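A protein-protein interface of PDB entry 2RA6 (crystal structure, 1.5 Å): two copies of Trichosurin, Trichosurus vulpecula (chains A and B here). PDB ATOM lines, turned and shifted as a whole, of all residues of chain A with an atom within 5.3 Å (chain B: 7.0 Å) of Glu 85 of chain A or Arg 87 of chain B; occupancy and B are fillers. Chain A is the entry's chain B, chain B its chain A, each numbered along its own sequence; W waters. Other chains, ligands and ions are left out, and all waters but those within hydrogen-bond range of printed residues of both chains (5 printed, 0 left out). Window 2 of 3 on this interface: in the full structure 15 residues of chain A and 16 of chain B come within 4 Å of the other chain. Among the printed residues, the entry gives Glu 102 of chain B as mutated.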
ATOM      1  N   THR A  83      26.052  25.847 -15.764  1.00  0.00           N
ATOM      2  CA  THR A  83      25.960  24.416 -15.503  1.00  0.00           C
ATOM      3  C   THR A  83      27.033  23.734 -16.338  1.00  0.00           C
ATOM      4  O   THR A  83      27.810  24.401 -17.018  1.00  0.00           O
ATOM      5  CB  THR A  83      24.589  23.851 -15.917  1.00  0.00           C
ATOM      6  OG1 THR A  83      24.464  23.900 -17.343  1.00  0.00           O
ATOM      7  CG2 THR A  83      23.465  24.661 -15.285  1.00  0.00           C
ATOM      8  N   GLU A  84      27.069  22.408 -16.291  1.00  0.00           N
ATOM      9  CA  GLU A  84      28.052  21.648 -17.058  1.00  0.00           C
ATOM     10  C   GLU A  84      27.777  21.786 -18.550  1.00  0.00           C
ATOM     11  O   GLU A  84      28.637  21.490 -19.380  1.00  0.00           O
ATOM     12  CB  GLU A  84      27.998  20.172 -16.662  1.00  0.00           C
ATOM     13  CG  GLU A  84      28.280  19.913 -15.194  1.00  0.00           C
ATOM     14  CD  GLU A  84      28.056  18.464 -14.808  1.00  0.00           C
ATOM     15  OE1 GLU A  84      28.739  17.583 -15.375  1.00  0.00           O
ATOM     16  OE2 GLU A  84      27.195  18.208 -13.938  1.00  0.00           O
ATOM     17  N   GLU A  85      26.574  22.240 -18.884  1.00  0.00           N
ATOM     18  CA  GLU A  85      26.172  22.415 -20.275  1.00  0.00           C
ATOM     19  C   GLU A  85      26.193  23.884 -20.681  1.00  0.00           C
ATOM     20  O   GLU A  85      25.638  24.740 -19.991  1.00  0.00           O
ATOM     21  CB  GLU A  85      24.766  21.844 -20.491  1.00  0.00           C
ATOM     22  CG  GLU A  85      24.651  20.337 -20.279  1.00  0.00           C
ATOM     23  CD  GLU A  85      25.280  19.530 -21.404  1.00  0.00           C
ATOM     24  OE1 GLU A  85      26.470  19.753 -21.709  1.00  0.00           O
ATOM     25  OE2 GLU A  85      24.583  18.669 -21.983  1.00  0.00           O
ATOM     26  N   ALA A  86      26.835  24.172 -21.806  1.00  0.00           N
ATOM     27  CA  ALA A  86      26.907  25.541 -22.290  1.00  0.00           C
ATOM     28  C   ALA A  86      25.498  26.060 -22.562  1.00  0.00           C
ATOM     29  O   ALA A  86      24.585  25.286 -22.847  1.00  0.00           O
ATOM     30  CB  ALA A  86      27.745  25.606 -23.563  1.00  0.00           C
ATOM     31  N   ARG A  87      25.346  27.375 -22.462  1.00  0.00           N
ATOM     32  CA  ARG A  87      24.082  28.067 -22.691  1.00  0.00           C
ATOM     33  C   ARG A  87      22.946  27.643 -21.763  1.00  0.00           C
ATOM     34  O   ARG A  87      21.814  28.092 -21.927  1.00  0.00           O
ATOM     35  CB  ARG A  87      23.647  27.921 -24.155  1.00  0.00           C
ATOM     36  CG  ARG A  87      22.929  26.636 -24.489  1.00  0.00           C
ATOM     37  CD  ARG A  87      22.679  26.517 -25.984  1.00  0.00           C
ATOM     38  NE  ARG A  87      21.929  25.306 -26.301  1.00  0.00           N
ATOM     39  CZ  ARG A  87      20.676  25.084 -25.919  1.00  0.00           C
ATOM     40  NH1 ARG A  87      20.030  25.998 -25.203  1.00  0.00           N
ATOM     41  NH2 ARG A  87      20.071  23.953 -26.253  1.00  0.00           N
ATOM     42  N   GLN A  88      23.239  26.778 -20.800  1.00  0.00           N
ATOM     43  CA  GLN A  88      22.228  26.347 -19.838  1.00  0.00           C
ATOM     44  C   GLN A  88      22.617  26.893 -18.469  1.00  0.00           C
ATOM     45  O   GLN A  88      23.771  26.774 -18.050  1.00  0.00           O
ATOM     46  CB  GLN A  88      22.140  24.825 -19.764  1.00  0.00           C
ATOM     47  CG  GLN A  88      20.932  24.338 -18.970  1.00  0.00           C
ATOM     48  CD  GLN A  88      20.892  22.833 -18.824  1.00  0.00           C
ATOM     49  OE1 GLN A  88      21.284  22.102 -19.734  1.00  0.00           O
ATOM     50  NE2 GLN A  88      20.397  22.359 -17.681  1.00  0.00           N
ATOM     51  N   TYR A 100      17.667  28.503 -20.575  1.00  0.00           N
ATOM     52  CA  TYR A 100      18.423  28.241 -21.796  1.00  0.00           C
ATOM     53  C   TYR A 100      18.549  29.505 -22.635  1.00  0.00           C
ATOM     54  O   TYR A 100      17.573  30.215 -22.866  1.00  0.00           O
ATOM     55  CB  TYR A 100      17.759  27.144 -22.636  1.00  0.00           C
ATOM     56  CG  TYR A 100      17.790  25.766 -22.011  1.00  0.00           C
ATOM     57  CD1 TYR A 100      16.821  25.376 -21.089  1.00  0.00           C
ATOM     58  CD2 TYR A 100      18.791  24.857 -22.342  1.00  0.00           C
ATOM     59  CE1 TYR A 100      16.850  24.107 -20.511  1.00  0.00           C
ATOM     60  CE2 TYR A 100      18.830  23.591 -21.771  1.00  0.00           C
ATOM     61  CZ  TYR A 100      17.858  23.221 -20.858  1.00  0.00           C
ATOM     62  OH  TYR A 100      17.897  21.967 -20.291  1.00  0.00           O
ATOM     63  N   THR B  83      18.114  20.551 -34.308  1.00  0.00           N
ATOM     64  CA  THR B  83      17.774  21.967 -34.354  1.00  0.00           C
ATOM     65  C   THR B  83      19.060  22.748 -34.576  1.00  0.00           C
ATOM     66  O   THR B  83      20.132  22.161 -34.718  1.00  0.00           O
ATOM     67  CB  THR B  83      17.136  22.443 -33.032  1.00  0.00           C
ATOM     68  OG1 THR B  83      18.113  22.395 -31.984  1.00  0.00           O
ATOM     69  CG2 THR B  83      15.959  21.558 -32.664  1.00  0.00           C
ATOM     70  N   GLU B  85      20.498  24.258 -32.497  1.00  0.00           N
ATOM     71  CA  GLU B  85      21.243  24.142 -31.252  1.00  0.00           C
ATOM     72  C   GLU B  85      21.742  22.718 -31.023  1.00  0.00           C
ATOM     73  O   GLU B  85      20.987  21.753 -31.143  1.00  0.00           O
ATOM     74  CB  GLU B  85      20.358  24.573 -30.080  1.00  0.00           C
ATOM     75  CG  GLU B  85      21.073  25.415 -29.039  1.00  0.00           C
ATOM     76  CD  GLU B  85      21.470  26.785 -29.560  1.00  0.00           C
ATOM     77  OE1 GLU B  85      20.572  27.555 -29.965  1.00  0.00           O
ATOM     78  OE2 GLU B  85      22.680  27.093 -29.561  1.00  0.00           O
ATOM     79  N   ALA B  86      23.022  22.590 -30.696  1.00  0.00           N
ATOM     80  CA  ALA B  86      23.604  21.281 -30.451  1.00  0.00           C
ATOM     81  C   ALA B  86      22.905  20.613 -29.272  1.00  0.00           C
ATOM     82  O   ALA B  86      22.463  21.284 -28.340  1.00  0.00           O
ATOM     83  CB  ALA B  86      25.098  21.415 -30.167  1.00  0.00           C
ATOM     84  N   ARG B  87      22.813  19.289 -29.332  1.00  0.00           N
ATOM     85  CA  ARG B  87      22.193  18.474 -28.290  1.00  0.00           C
ATOM     86  C   ARG B  87      20.716  18.781 -28.035  1.00  0.00           C
ATOM     87  O   ARG B  87      20.123  18.252 -27.100  1.00  0.00           O
ATOM     88  CB  ARG B  87      22.990  18.586 -26.980  1.00  0.00           C
ATOM     89  CG  ARG B  87      22.636  19.771 -26.099  1.00  0.00           C
ATOM     90  CD  ARG B  87      23.638  19.949 -24.961  1.00  0.00           C
ATOM     91  NE  ARG B  87      23.217  20.999 -24.038  1.00  0.00           N
ATOM     92  CZ  ARG B  87      22.157  20.910 -23.242  1.00  0.00           C
ATOM     93  NH1 ARG B  87      21.413  19.810 -23.254  1.00  0.00           N
ATOM     94  NH2 ARG B  87      21.834  21.922 -22.444  1.00  0.00           N
ATOM     95  N   GLN B  88      20.124  19.638 -28.856  1.00  0.00           N
ATOM     96  CA  GLN B  88      18.712  19.957 -28.704  1.00  0.00           C
ATOM     97  C   GLN B  88      17.968  19.415 -29.915  1.00  0.00           C
ATOM     98  O   GLN B  88      18.413  19.573 -31.054  1.00  0.00           O
ATOM     99  CB  GLN B  88      18.494  21.463 -28.594  1.00  0.00           C
ATOM    100  CG  GLN B  88      17.025  21.836 -28.454  1.00  0.00           C
ATOM    101  CD  GLN B  88      16.806  23.320 -28.245  1.00  0.00           C
ATOM    102  OE1 GLN B  88      15.680  23.812 -28.339  1.00  0.00           O
ATOM    103  NE2 GLN B  88      17.879  24.042 -27.955  1.00  0.00           N
ATOM    104  N   PHE B  89      16.837  18.770 -29.665  1.00  0.00           N
ATOM    105  CA  PHE B  89      16.049  18.197 -30.742  1.00  0.00           C
ATOM    106  C   PHE B  89      14.585  18.563 -30.585  1.00  0.00           C
ATOM    107  O   PHE B  89      14.163  19.073 -29.544  1.00  0.00           O
ATOM    108  CB  PHE B  89      16.186  16.672 -30.750  1.00  0.00           C
ATOM    109  CG  PHE B  89      17.604  16.196 -30.782  1.00  0.00           C
ATOM    110  CD1 PHE B  89      18.372  16.189 -29.624  1.00  0.00           C
ATOM    111  CD2 PHE B  89      18.185  15.779 -31.975  1.00  0.00           C
ATOM    112  CE1 PHE B  89      19.700  15.775 -29.649  1.00  0.00           C
ATOM    113  CE2 PHE B  89      19.515  15.362 -32.013  1.00  0.00           C
ATOM    114  CZ  PHE B  89      20.274  15.361 -30.844  1.00  0.00           C
ATOM    115  N   VAL B  99      13.518  18.541 -26.811  1.00  0.00           N
ATOM    116  CA  VAL B  99      14.338  17.481 -26.232  1.00  0.00           C
ATOM    117  C   VAL B  99      15.791  17.884 -26.071  1.00  0.00           C
ATOM    118  O   VAL B  99      16.407  18.395 -27.008  1.00  0.00           O
ATOM    119  CB  VAL B  99      14.292  16.213 -27.119  1.00  0.00           C
ATOM    120  CG1 VAL B  99      15.032  15.077 -26.439  1.00  0.00           C
ATOM    121  CG2 VAL B  99      12.847  15.826 -27.416  1.00  0.00           C
ATOM    122  N   TYR B 100      16.337  17.652 -24.880  1.00  0.00           N
ATOM    123  CA  TYR B 100      17.732  17.983 -24.602  1.00  0.00           C
ATOM    124  C   TYR B 100      18.512  16.737 -24.192  1.00  0.00           C
ATOM    125  O   TYR B 100      18.081  15.979 -23.326  1.00  0.00           O
ATOM    126  CB  TYR B 100      17.827  19.019 -23.479  1.00  0.00           C
ATOM    127  CG  TYR B 100      17.285  20.372 -23.853  1.00  0.00           C
ATOM    128  CD1 TYR B 100      18.094  21.314 -24.489  1.00  0.00           C
ATOM    129  CD2 TYR B 100      15.963  20.708 -23.577  1.00  0.00           C
ATOM    130  CE1 TYR B 100      17.594  22.566 -24.840  1.00  0.00           C
ATOM    131  CE2 TYR B 100      15.448  21.955 -23.922  1.00  0.00           C
ATOM    132  CZ  TYR B 100      16.272  22.877 -24.551  1.00  0.00           C
ATOM    133  OH  TYR B 100      15.769  24.115 -24.883  1.00  0.00           O
ATOM    134  N   TYR B 101      19.657  16.530 -24.828  1.00  0.00           N
ATOM    135  CA  TYR B 101      20.521  15.396 -24.525  1.00  0.00           C
ATOM    136  C   TYR B 101      21.680  15.839 -23.637  1.00  0.00           C
ATOM    137  O   TYR B 101      22.234  16.926 -23.824  1.00  0.00           O
ATOM    138  CB  TYR B 101      21.085  14.803 -25.821  1.00  0.00           C
ATOM    139  CG  TYR B 101      22.273  13.887 -25.626  1.00  0.00           C
ATOM    140  CD1 TYR B 101      22.116  12.606 -25.105  1.00  0.00           C
ATOM    141  CD2 TYR B 101      23.558  14.304 -25.971  1.00  0.00           C
ATOM    142  CE1 TYR B 101      23.209  11.753 -24.934  1.00  0.00           C
ATOM    143  CE2 TYR B 101      24.657  13.463 -25.807  1.00  0.00           C
ATOM    144  CZ  TYR B 101      24.473  12.188 -25.288  1.00  0.00           C
ATOM    145  OH  TYR B 101      25.556  11.347 -25.141  1.00  0.00           O
ATOM    146  N   GLU B 102      22.034  14.993 -22.671  1.00  0.00           N
ATOM    147  CA  GLU B 102      23.146  15.261 -21.756  1.00  0.00           C
ATOM    148  C   GLU B 102      23.808  13.941 -21.356  1.00  0.00           C
ATOM    149  O   GLU B 102      23.135  12.920 -21.260  1.00  0.00           O
ATOM    150  CB  GLU B 102      22.648  15.949 -20.479  1.00  0.00           C
ATOM    151  CG  GLU B 102      22.025  17.325 -20.658  1.00  0.00           C
ATOM    152  CD  GLU B 102      21.536  17.902 -19.338  1.00  0.00           C
ATOM    153  OE1 GLU B 102      22.342  17.962 -18.381  1.00  0.00           O
ATOM    154  OE2 GLU B 102      20.351  18.297 -19.252  1.00  0.00           O
ATOM    155  N   SER B 103      25.122  13.967 -21.137  1.00  0.00           N
ATOM    156  CA  SER B 103      25.869  12.784 -20.692  1.00  0.00           C
ATOM    157  C   SER B 103      27.349  13.055 -20.478  1.00  0.00           C
ATOM    158  O   SER B 103      28.039  13.507 -21.388  1.00  0.00           O
ATOM    159  CB  SER B 103      25.751  11.627 -21.683  1.00  0.00           C
ATOM    160  OG  SER B 103      26.492  10.513 -21.200  1.00  0.00           O
ATOM    161  N   PHE B 112      18.020  12.096 -21.425  1.00  0.00           N
ATOM    162  CA  PHE B 112      17.202  12.901 -22.321  1.00  0.00           C
ATOM    163  C   PHE B 112      16.130  13.580 -21.494  1.00  0.00           C
ATOM    164  O   PHE B 112      15.412  12.928 -20.739  1.00  0.00           O
ATOM    165  CB  PHE B 112      16.533  12.047 -23.406  1.00  0.00           C
ATOM    166  CG  PHE B 112      17.466  11.613 -24.502  1.00  0.00           C
ATOM    167  CD1 PHE B 112      18.085  10.369 -24.452  1.00  0.00           C
ATOM    168  CD2 PHE B 112      17.722  12.449 -25.589  1.00  0.00           C
ATOM    169  CE1 PHE B 112      18.943   9.959 -25.467  1.00  0.00           C
ATOM    170  CE2 PHE B 112      18.583  12.046 -26.610  1.00  0.00           C
ATOM    171  CZ  PHE B 112      19.191  10.800 -26.546  1.00  0.00           C
ATOM    172  N   ILE B 113      16.056  14.894 -21.623  1.00  0.00           N
ATOM    173  CA  ILE B 113      15.065  15.688 -20.918  1.00  0.00           C
ATOM    174  C   ILE B 113      14.054  16.139 -21.964  1.00  0.00           C
ATOM    175  O   ILE B 113      14.417  16.735 -22.983  1.00  0.00           O
ATOM    176  CB  ILE B 113      15.700  16.928 -20.262  1.00  0.00           C
ATOM    177  CG1 ILE B 113      16.834  16.504 -19.317  1.00  0.00           C
ATOM    178  CG2 ILE B 113      14.634  17.725 -19.520  1.00  0.00           C
ATOM    179  CD1 ILE B 113      16.452  15.428 -18.314  1.00  0.00           C
HETATM  180  O   HOH W   1      26.649  16.236 -22.713  1.00  0.00           O
HETATM  181  O   HOH W   2      20.155  20.236 -21.072  1.00  0.00           O
HETATM  182  O   HOH W   3      20.067  19.287 -16.782  1.00  0.00           O
HETATM  183  O   HOH W   4      24.898  23.089 -24.672  1.00  0.00           O
HETATM  184  O   HOH W   5      17.578  25.970 -25.950  1.00  0.00           O
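Printed residues of chain B that touch a printed residue of chain A: Glu 85, Arg 87, Gln 88, Tyr 100, Tyr 101 and Glu 102.
Among the printed residues, 10 pairs touch across the chains.
Among the printed residues, Asp or Glu carboxylates within 4 Å of a Lys or Arg side-chain nitrogen of the other chain: Glu 85 of chain A with Arg 87 of chain B and Arg 87 of chain A with Glu 85 of chain B.
The side-chain hydroxyl of Thr 83 of chain B lies within hydrogen-bond range of the backbone carbonyl oxygen of Glu 85 of chain B, 3.1 Å away.
OG1 of Thr 83 of chain B sits at hydrogen-bond distance from O of Gln 88 of chain B (3.0 Å).
The backbone carbonyl oxygen (O) of Arg 87 of chain B is in hydrogen-bond range of the backbone NH (N) of Tyr 101 of chain B (2.9 Å).
OH of Tyr 100 of chain B sits at hydrogen-bond distance from OE1 of Gln 88 of chain B (3.5 Å).
O of Gln 88 of chain A is in hydrogen-bond range of OG1 of Thr 83 of chain A.
OE1 of Gln 88 of chain A is in hydrogen-bond range of OH of Tyr 100 of chain A.
CG of Glu 102 of chain B touches OE2 of Glu 85 of chain A, 3.2 Å away.
NH2 of Arg 87 of chain A touches CE1 of Tyr 100 of chain B, at 3.2 Å.
Gln 88 of chain A touches Glu 102 of chain B (OE1 to OE2, 3.9 Å).
CE2 of Tyr 100 of chain A touches NH2 of Arg 87 of chain B, 3.5 Å away.
Tyr 100 of chain B touches Tyr 100 of chain A (CE1 to CE2, 3.5 Å).
Water W2 lies within hydrogen-bond range of the guanidinium group of Arg 87 of chain B (2.6 Å), the side-chain amide oxygen of Gln 88 of chain A (2.6 Å), the side-chain carboxylate of Glu 102 of chain B (2.7 Å) and the side-chain hydroxyl of Tyr 100 of chain A (3.0 Å).
Water W5 lies within hydrogen-bond range of the guanidinium group (NH1) of Arg 87 of chain A, the side-chain amide nitrogen (NE2) of Gln 88 of chain B and the side-chain hydroxyl (OH) of Tyr 100 of chain B.
Water W3 bridges the side-chain carboxylate of Glu 102 of chain B (2.7 Å) and the side-chain amide nitrogen of Gln 88 of chain A (3.2 Å).
Water W4 lies within hydrogen-bond range of NE of Arg 87 of chain B (2.8 Å) and O of Ala 86 of chain A (2.9 Å).
Water W1 bridges the backbone NH of Ser 103 of chain B and the side-chain carboxylate of Glu 85 of chain A.
Glu 85 of chain A touches Arg 87 of chain B, and with the chains exchanged Arg 87 of chain A touches Glu 85 of chain B.
Arg 87 of chain A touches Gln 88 of chain B, and with the chains exchanged Gln 88 of chain A touches Arg 87 of chain B.
Arg 87 of chain A touches Tyr 100 of chain B, and with the chains exchanged Tyr 100 of chain A touches Arg 87 of chain B.
Tyr 100 of chain A touches its own counterpart, Tyr 100 of chain B.
Positions printed for both chains: 83, 85, 86, 87, 88 and 100.
Of chain B, only Arg 87, Tyr 101 and Glu 102 come within 4 Å of Glu 85 of chain A.
Printed residues of chain A within 4 Å of Glu 85 of chain B: Arg 87 (2.9 Å).
Of chain A, only Glu 85, Gln 88 and Tyr 100 come within 4 Å of Arg 87 of chain B.
Of the printed residues of chain A, Gln 88 of chain B touches Arg 87 (2.8 Å).
Printed residues of chain A within 4 Å of Tyr 100 of chain B: Arg 87 and Tyr 100.
Printed residues of chain A within 4 Å of Glu 102 of chain B: Glu 85 and Gln 88.
The side-chain carboxylate (OE2) of Glu 85 of chain B is in salt-bridge range of the guanidinium group (NE) of Arg 87 of chain A.
NE of Arg 87 of chain B is in salt-bridge range of OE2 of Glu 85 of chain A, at 3.4 Å.
The side-chain amide oxygen (OE1) of Gln 88 of chain A is in hydrogen-bond range of the guanidinium group (NH2) of Arg 87 of chain B (2.8 Å).
The side-chain amide nitrogen (NE2) of Gln 88 of chain B lies close to the guanidinium group (NH2) of Arg 87 of chain A.
O of Tyr 101 of chain B lies close to OE2 of Glu 85 of chain A (3.5 Å).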
